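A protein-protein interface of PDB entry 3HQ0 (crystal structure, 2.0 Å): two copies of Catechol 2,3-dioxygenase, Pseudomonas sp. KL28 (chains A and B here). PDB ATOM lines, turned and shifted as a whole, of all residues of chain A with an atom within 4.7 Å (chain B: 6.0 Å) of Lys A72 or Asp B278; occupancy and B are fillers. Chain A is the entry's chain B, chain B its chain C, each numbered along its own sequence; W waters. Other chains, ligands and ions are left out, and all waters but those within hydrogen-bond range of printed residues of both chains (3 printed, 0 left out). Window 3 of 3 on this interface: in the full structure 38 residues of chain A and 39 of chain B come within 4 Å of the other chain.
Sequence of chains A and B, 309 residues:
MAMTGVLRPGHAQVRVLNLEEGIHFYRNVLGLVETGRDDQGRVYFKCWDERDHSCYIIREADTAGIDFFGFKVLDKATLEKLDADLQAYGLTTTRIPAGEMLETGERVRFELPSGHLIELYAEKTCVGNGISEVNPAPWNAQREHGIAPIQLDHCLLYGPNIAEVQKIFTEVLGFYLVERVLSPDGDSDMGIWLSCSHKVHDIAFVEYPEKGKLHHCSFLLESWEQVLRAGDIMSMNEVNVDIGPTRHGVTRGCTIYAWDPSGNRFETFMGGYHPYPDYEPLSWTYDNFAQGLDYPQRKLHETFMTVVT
Of the printed residues of chain B, Arg A8 touches Tyr B276 (3.3 Å) and Asp B278 (2.9 Å). Lys A72 touches just one residue of chain B: Asp B278 (3.3 Å). Of the printed residues of chain A, Tyr B276 touches Leu A7 (3.4 Å) and Arg A8 (3.3 Å). Of chain A, only Leu A7, Arg A8 and Lys A72 come within 4 Å of Asp B278. Glu B280 touches none of the printed residues of chain A.
Water W3 lies within hydrogen-bond range of the side-chain carboxylate of Asp B278 (2.5 Å), the side-chain carboxylate of Asp A52 (2.8 Å) and the side-chain amino group of Lys A72 (3.3 Å). Water W1 bridges OH of Tyr B276 and O of Leu A7. Water W2 bridges the side-chain hydroxyl (OH) of Tyr B279 (2.8 Å) and the backbone NH (N) of Asp A52 (3.0 Å).
OD2 of Asp B278 is in salt-bridge range of NZ of Lys A72, 3.3 Å away. The guanidinium group (NH1) of Arg A8 lies within salt-bridge range of the side-chain carboxylate (OD1) of Asp B278 (2.9 Å).
The guanidinium group (NH2) of Arg A8 lies within salt-bridge range of the side-chain carboxylate (OD2) of Asp A52, 3.2 Å away. N of Leu A7 is in hydrogen-bond range of O of Lys A72 (2.8 Å). O of Gly A5 lies within hydrogen-bond range of N of Leu A74 (2.8 Å). The side-chain carboxylate (OD2) of Asp A52 is in salt-bridge range of the side-chain amino group (NZ) of Lys A72, at 2.7 Å. The side-chain hydroxyl (OH) of Tyr B176 lies within hydrogen-bond range of the backbone NH (N) of Tyr B276. The backbone NH (N) of Lys A72 is in hydrogen-bond range of the backbone carbonyl oxygen (O) of Arg A8 (3.0 Å).
Printed residues of chain B that touch a printed residue of chain A: Tyr B276, Pro B277 and Asp B278. Hydrophobic or aromatic side chains of chain B within 4 Å of the printed part of chain A: Tyr B276 and Pro B277. Of the 15 printed residues of chain A, 4 touch a printed residue of chain B. Hydrophobic or aromatic side chains of chain A that line the printed part of chain B: Leu A7 and Leu A74.
Tyr B276 touches Leu A7 (CE1 to O, 3.4 Å). Leu A7 touches Asp B278. Arg A8 touches Tyr B276. CD1 of Leu A74 touches CB of Pro B277 (3.99 Å).
No position is printed for both chains.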
ATOM      1  N   GLY A   5      -1.750 -26.617 -21.447  1.00  0.00           N
ATOM      2  CA  GLY A   5      -3.126 -26.733 -21.902  1.00  0.00           C
ATOM      3  C   GLY A   5      -4.095 -26.387 -20.784  1.00  0.00           C
ATOM      4  O   GLY A   5      -4.046 -25.283 -20.246  1.00  0.00           O
ATOM      5  N   VAL A   6      -4.977 -27.319 -20.431  1.00  0.00           N
ATOM      6  CA  VAL A   6      -5.948 -27.083 -19.353  1.00  0.00           C
ATOM      7  C   VAL A   6      -5.225 -27.430 -18.069  1.00  0.00           C
ATOM      8  O   VAL A   6      -4.770 -28.563 -17.903  1.00  0.00           O
ATOM      9  CB  VAL A   6      -7.183 -27.995 -19.495  1.00  0.00           C
ATOM     10  CG1 VAL A   6      -8.213 -27.667 -18.388  1.00  0.00           C
ATOM     11  CG2 VAL A   6      -7.796 -27.815 -20.864  1.00  0.00           C
ATOM     12  N   LEU A   7      -5.113 -26.469 -17.156  1.00  0.00           N
ATOM     13  CA  LEU A   7      -4.374 -26.707 -15.924  1.00  0.00           C
ATOM     14  C   LEU A   7      -5.144 -27.246 -14.732  1.00  0.00           C
ATOM     15  O   LEU A   7      -4.695 -28.190 -14.068  1.00  0.00           O
ATOM     16  CB  LEU A   7      -3.667 -25.422 -15.472  1.00  0.00           C
ATOM     17  CG  LEU A   7      -2.767 -24.642 -16.435  1.00  0.00           C
ATOM     18  CD1 LEU A   7      -2.237 -23.395 -15.706  1.00  0.00           C
ATOM     19  CD2 LEU A   7      -1.619 -25.523 -16.924  1.00  0.00           C
ATOM     20  N   ARG A   8      -6.301 -26.657 -14.448  1.00  0.00           N
ATOM     21  CA  ARG A   8      -7.038 -27.076 -13.261  1.00  0.00           C
ATOM     22  C   ARG A   8      -8.444 -26.496 -13.166  1.00  0.00           C
ATOM     23  O   ARG A   8      -8.788 -25.535 -13.866  1.00  0.00           O
ATOM     24  CB  ARG A   8      -6.268 -26.586 -12.036  1.00  0.00           C
ATOM     25  CG  ARG A   8      -6.079 -25.053 -12.068  1.00  0.00           C
ATOM     26  CD  ARG A   8      -5.541 -24.490 -10.759  1.00  0.00           C
ATOM     27  NE  ARG A   8      -5.506 -23.024 -10.731  1.00  0.00           N
ATOM     28  CZ  ARG A   8      -4.529 -22.270 -11.226  1.00  0.00           C
ATOM     29  NH1 ARG A   8      -3.475 -22.821 -11.807  1.00  0.00           N
ATOM     30  NH2 ARG A   8      -4.596 -20.952 -11.117  1.00  0.00           N
ATOM     31  N   PRO A   9      -9.281 -27.075 -12.290  1.00  0.00           N
ATOM     32  CA  PRO A   9     -10.624 -26.509 -12.170  1.00  0.00           C
ATOM     33  C   PRO A   9     -10.371 -25.064 -11.732  1.00  0.00           C
ATOM     34  O   PRO A   9      -9.526 -24.824 -10.868  1.00  0.00           O
ATOM     35  CB  PRO A   9     -11.254 -27.362 -11.076  1.00  0.00           C
ATOM     36  CG  PRO A   9     -10.613 -28.729 -11.323  1.00  0.00           C
ATOM     37  CD  PRO A   9      -9.171 -28.368 -11.583  1.00  0.00           C
ATOM     38  N   GLY A  10     -11.062 -24.108 -12.351  1.00  0.00           N
ATOM     39  CA  GLY A  10     -10.861 -22.703 -12.018  1.00  0.00           C
ATOM     40  C   GLY A  10     -11.992 -22.055 -11.234  1.00  0.00           C
ATOM     41  O   GLY A  10     -11.760 -21.220 -10.350  1.00  0.00           O
ATOM     42  N   ASP A  52      -5.594 -17.399  -6.789  1.00  0.00           N
ATOM     43  CA  ASP A  52      -6.467 -16.646  -7.688  1.00  0.00           C
ATOM     44  C   ASP A  52      -7.699 -16.106  -6.990  1.00  0.00           C
ATOM     45  O   ASP A  52      -8.167 -16.666  -6.002  1.00  0.00           O
ATOM     46  CB  ASP A  52      -6.868 -17.493  -8.894  1.00  0.00           C
ATOM     47  CG  ASP A  52      -5.794 -17.514  -9.958  1.00  0.00           C
ATOM     48  OD1 ASP A  52      -4.708 -16.950  -9.713  1.00  0.00           O
ATOM     49  OD2 ASP A  52      -6.023 -18.093 -11.035  1.00  0.00           O
ATOM     50  N   GLY A  70     -15.769 -23.728 -14.753  1.00  0.00           N
ATOM     51  CA  GLY A  70     -14.650 -23.250 -15.550  1.00  0.00           C
ATOM     52  C   GLY A  70     -13.281 -23.801 -15.189  1.00  0.00           C
ATOM     53  O   GLY A  70     -13.026 -24.164 -14.036  1.00  0.00           O
ATOM     54  N   PHE A  71     -12.402 -23.865 -16.186  1.00  0.00           N
ATOM     55  CA  PHE A  71     -11.041 -24.362 -16.019  1.00  0.00           C
ATOM     56  C   PHE A  71     -10.048 -23.286 -16.432  1.00  0.00           C
ATOM     57  O   PHE A  71     -10.301 -22.517 -17.363  1.00  0.00           O
ATOM     58  CB  PHE A  71     -10.807 -25.603 -16.892  1.00  0.00           C
ATOM     59  CG  PHE A  71     -11.500 -26.843 -16.402  1.00  0.00           C
ATOM     60  CD1 PHE A  71     -10.912 -27.646 -15.427  1.00  0.00           C
ATOM     61  CD2 PHE A  71     -12.730 -27.221 -16.929  1.00  0.00           C
ATOM     62  CE1 PHE A  71     -11.538 -28.816 -14.983  1.00  0.00           C
ATOM     63  CE2 PHE A  71     -13.367 -28.383 -16.497  1.00  0.00           C
ATOM     64  CZ  PHE A  71     -12.766 -29.187 -15.518  1.00  0.00           C
ATOM     65  N   LYS A  72      -8.914 -23.216 -15.743  1.00  0.00           N
ATOM     66  CA  LYS A  72      -7.915 -22.231 -16.111  1.00  0.00           C
ATOM     67  C   LYS A  72      -6.957 -22.935 -17.045  1.00  0.00           C
ATOM     68  O   LYS A  72      -6.624 -24.106 -16.841  1.00  0.00           O
ATOM     69  CB  LYS A  72      -7.163 -21.700 -14.884  1.00  0.00           C
ATOM     70  CG  LYS A  72      -6.132 -20.608 -15.240  1.00  0.00           C
ATOM     71  CD  LYS A  72      -5.697 -19.798 -14.024  1.00  0.00           C
ATOM     72  CE  LYS A  72      -4.795 -18.616 -14.415  1.00  0.00           C
ATOM     73  NZ  LYS A  72      -4.589 -17.662 -13.275  1.00  0.00           N
ATOM     74  N   VAL A  73      -6.545 -22.239 -18.097  1.00  0.00           N
ATOM     75  CA  VAL A  73      -5.606 -22.816 -19.049  1.00  0.00           C
ATOM     76  C   VAL A  73      -4.275 -22.079 -18.932  1.00  0.00           C
ATOM     77  O   VAL A  73      -4.206 -20.997 -18.359  1.00  0.00           O
ATOM     78  CB  VAL A  73      -6.152 -22.727 -20.485  1.00  0.00           C
ATOM     79  CG1 VAL A  73      -7.525 -23.368 -20.539  1.00  0.00           C
ATOM     80  CG2 VAL A  73      -6.212 -21.269 -20.944  1.00  0.00           C
ATOM     81  N   LEU A  74      -3.224 -22.667 -19.488  1.00  0.00           N
ATOM     82  CA  LEU A  74      -1.885 -22.103 -19.398  1.00  0.00           C
ATOM     83  C   LEU A  74      -1.753 -20.634 -19.776  1.00  0.00           C
ATOM     84  O   LEU A  74      -1.240 -19.828 -18.994  1.00  0.00           O
ATOM     85  CB  LEU A  74      -0.918 -22.938 -20.245  1.00  0.00           C
ATOM     86  CG  LEU A  74       0.565 -22.603 -20.075  1.00  0.00           C
ATOM     87  CD1 LEU A  74       1.042 -23.094 -18.720  1.00  0.00           C
ATOM     88  CD2 LEU A  74       1.362 -23.255 -21.181  1.00  0.00           C
ATOM     89  N   TYR A 121     -10.613 -20.310 -19.390  1.00  0.00           N
ATOM     90  CA  TYR A 121     -10.100 -18.955 -19.311  1.00  0.00           C
ATOM     91  C   TYR A 121      -8.615 -19.004 -19.003  1.00  0.00           C
ATOM     92  O   TYR A 121      -8.127 -19.951 -18.383  1.00  0.00           O
ATOM     93  CB  TYR A 121     -10.834 -18.130 -18.246  1.00  0.00           C
ATOM     94  CG  TYR A 121     -10.641 -18.608 -16.822  1.00  0.00           C
ATOM     95  CD1 TYR A 121     -11.463 -19.599 -16.281  1.00  0.00           C
ATOM     96  CD2 TYR A 121      -9.656 -18.052 -16.009  1.00  0.00           C
ATOM     97  CE1 TYR A 121     -11.313 -20.019 -14.960  1.00  0.00           C
ATOM     98  CE2 TYR A 121      -9.494 -18.466 -14.686  1.00  0.00           C
ATOM     99  CZ  TYR A 121     -10.328 -19.446 -14.168  1.00  0.00           C
ATOM    100  OH  TYR A 121     -10.189 -19.839 -12.861  1.00  0.00           O
ATOM    101  N   ALA A 122      -7.896 -17.982 -19.440  1.00  0.00           N
ATOM    102  CA  ALA A 122      -6.467 -17.939 -19.215  1.00  0.00           C
ATOM    103  C   ALA A 122      -6.081 -16.958 -18.130  1.00  0.00           C
ATOM    104  O   ALA A 122      -5.014 -17.091 -17.529  1.00  0.00           O
ATOM    105  CB  ALA A 122      -5.752 -17.587 -20.507  1.00  0.00           C
ATOM    106  N   LYS A 124      -7.072 -14.564 -14.542  1.00  0.00           N
ATOM    107  CA  LYS A 124      -7.819 -14.251 -13.333  1.00  0.00           C
ATOM    108  C   LYS A 124      -6.773 -13.698 -12.373  1.00  0.00           C
ATOM    109  O   LYS A 124      -5.738 -14.327 -12.117  1.00  0.00           O
ATOM    110  CB  LYS A 124      -8.497 -15.484 -12.728  1.00  0.00           C
ATOM    111  CG  LYS A 124      -9.353 -15.145 -11.501  1.00  0.00           C
ATOM    112  CD  LYS A 124     -10.120 -16.351 -10.959  1.00  0.00           C
ATOM    113  CE  LYS A 124     -11.268 -16.767 -11.864  1.00  0.00           C
ATOM    114  NZ  LYS A 124     -11.964 -17.984 -11.338  1.00  0.00           N
ATOM    115  N   TYR B 176       9.731 -25.046 -13.846  1.00  0.00           N
ATOM    116  CA  TYR B 176       9.498 -23.685 -13.387  1.00  0.00           C
ATOM    117  C   TYR B 176       9.839 -23.584 -11.896  1.00  0.00           C
ATOM    118  O   TYR B 176       9.614 -24.524 -11.135  1.00  0.00           O
ATOM    119  CB  TYR B 176       8.049 -23.276 -13.653  1.00  0.00           C
ATOM    120  CG  TYR B 176       7.003 -23.974 -12.807  1.00  0.00           C
ATOM    121  CD1 TYR B 176       6.452 -23.341 -11.695  1.00  0.00           C
ATOM    122  CD2 TYR B 176       6.545 -25.253 -13.135  1.00  0.00           C
ATOM    123  CE1 TYR B 176       5.470 -23.955 -10.929  1.00  0.00           C
ATOM    124  CE2 TYR B 176       5.562 -25.881 -12.373  1.00  0.00           C
ATOM    125  CZ  TYR B 176       5.029 -25.221 -11.270  1.00  0.00           C
ATOM    126  OH  TYR B 176       4.060 -25.815 -10.505  1.00  0.00           O
ATOM    127  N   TYR B 276       1.249 -24.281  -9.637  1.00  0.00           N
ATOM    128  CA  TYR B 276       0.980 -24.490 -11.047  1.00  0.00           C
ATOM    129  C   TYR B 276       1.900 -23.498 -11.780  1.00  0.00           C
ATOM    130  O   TYR B 276       2.347 -22.508 -11.194  1.00  0.00           O
ATOM    131  CB  TYR B 276      -0.504 -24.232 -11.337  1.00  0.00           C
ATOM    132  CG  TYR B 276      -1.428 -25.389 -10.956  1.00  0.00           C
ATOM    133  CD1 TYR B 276      -1.696 -26.425 -11.855  1.00  0.00           C
ATOM    134  CD2 TYR B 276      -2.023 -25.451  -9.688  1.00  0.00           C
ATOM    135  CE1 TYR B 276      -2.543 -27.503 -11.502  1.00  0.00           C
ATOM    136  CE2 TYR B 276      -2.865 -26.520  -9.326  1.00  0.00           C
ATOM    137  CZ  TYR B 276      -3.120 -27.540 -10.238  1.00  0.00           C
ATOM    138  OH  TYR B 276      -3.954 -28.586  -9.891  1.00  0.00           O
ATOM    139  N   PRO B 277       2.206 -23.755 -13.062  1.00  0.00           N
ATOM    140  CA  PRO B 277       3.082 -22.900 -13.878  1.00  0.00           C
ATOM    141  C   PRO B 277       2.728 -21.409 -13.913  1.00  0.00           C
ATOM    142  O   PRO B 277       3.576 -20.571 -14.218  1.00  0.00           O
ATOM    143  CB  PRO B 277       3.000 -23.538 -15.267  1.00  0.00           C
ATOM    144  CG  PRO B 277       2.681 -24.959 -14.977  1.00  0.00           C
ATOM    145  CD  PRO B 277       1.678 -24.871 -13.862  1.00  0.00           C
ATOM    146  N   ASP B 278       1.485 -21.068 -13.611  1.00  0.00           N
ATOM    147  CA  ASP B 278       1.096 -19.669 -13.630  1.00  0.00           C
ATOM    148  C   ASP B 278       1.444 -18.938 -12.333  1.00  0.00           C
ATOM    149  O   ASP B 278       1.233 -17.738 -12.232  1.00  0.00           O
ATOM    150  CB  ASP B 278      -0.403 -19.529 -13.939  1.00  0.00           C
ATOM    151  CG  ASP B 278      -1.282 -20.251 -12.940  1.00  0.00           C
ATOM    152  OD1 ASP B 278      -1.125 -21.482 -12.787  1.00  0.00           O
ATOM    153  OD2 ASP B 278      -2.132 -19.585 -12.313  1.00  0.00           O
ATOM    154  N   TYR B 279       2.007 -19.664 -11.364  1.00  0.00           N
ATOM    155  CA  TYR B 279       2.378 -19.102 -10.060  1.00  0.00           C
ATOM    156  C   TYR B 279       3.768 -18.496  -9.985  1.00  0.00           C
ATOM    157  O   TYR B 279       4.706 -18.999 -10.595  1.00  0.00           O
ATOM    158  CB  TYR B 279       2.313 -20.175  -8.962  1.00  0.00           C
ATOM    159  CG  TYR B 279       0.932 -20.523  -8.480  1.00  0.00           C
ATOM    160  CD1 TYR B 279       0.754 -21.371  -7.391  1.00  0.00           C
ATOM    161  CD2 TYR B 279      -0.198 -20.016  -9.114  1.00  0.00           C
ATOM    162  CE1 TYR B 279      -0.518 -21.705  -6.940  1.00  0.00           C
ATOM    163  CE2 TYR B 279      -1.472 -20.341  -8.679  1.00  0.00           C
ATOM    164  CZ  TYR B 279      -1.628 -21.186  -7.590  1.00  0.00           C
ATOM    165  OH  TYR B 279      -2.894 -21.491  -7.150  1.00  0.00           O
ATOM    166  N   GLU B 280       3.894 -17.431  -9.198  1.00  0.00           N
ATOM    167  CA  GLU B 280       5.179 -16.781  -8.997  1.00  0.00           C
ATOM    168  C   GLU B 280       5.866 -17.524  -7.861  1.00  0.00           C
ATOM    169  O   GLU B 280       5.216 -17.963  -6.911  1.00  0.00           O
ATOM    170  CB  GLU B 280       4.995 -15.308  -8.628  1.00  0.00           C
ATOM    171  CG  GLU B 280       4.499 -14.449  -9.778  1.00  0.00           C
ATOM    172  CD  GLU B 280       5.225 -14.756 -11.077  1.00  0.00           C
ATOM    173  OE1 GLU B 280       6.476 -14.764 -11.078  1.00  0.00           O
ATOM    174  OE2 GLU B 280       4.550 -14.995 -12.101  1.00  0.00           O
HETATM  175  O   HOH W   1      -5.260 -29.841 -11.849  1.00  0.00           O
HETATM  176  O   HOH W   2      -5.403 -20.265  -7.624  1.00  0.00           O
HETATM  177  O   HOH W   3      -2.207 -17.517 -10.938  1.00  0.00           O
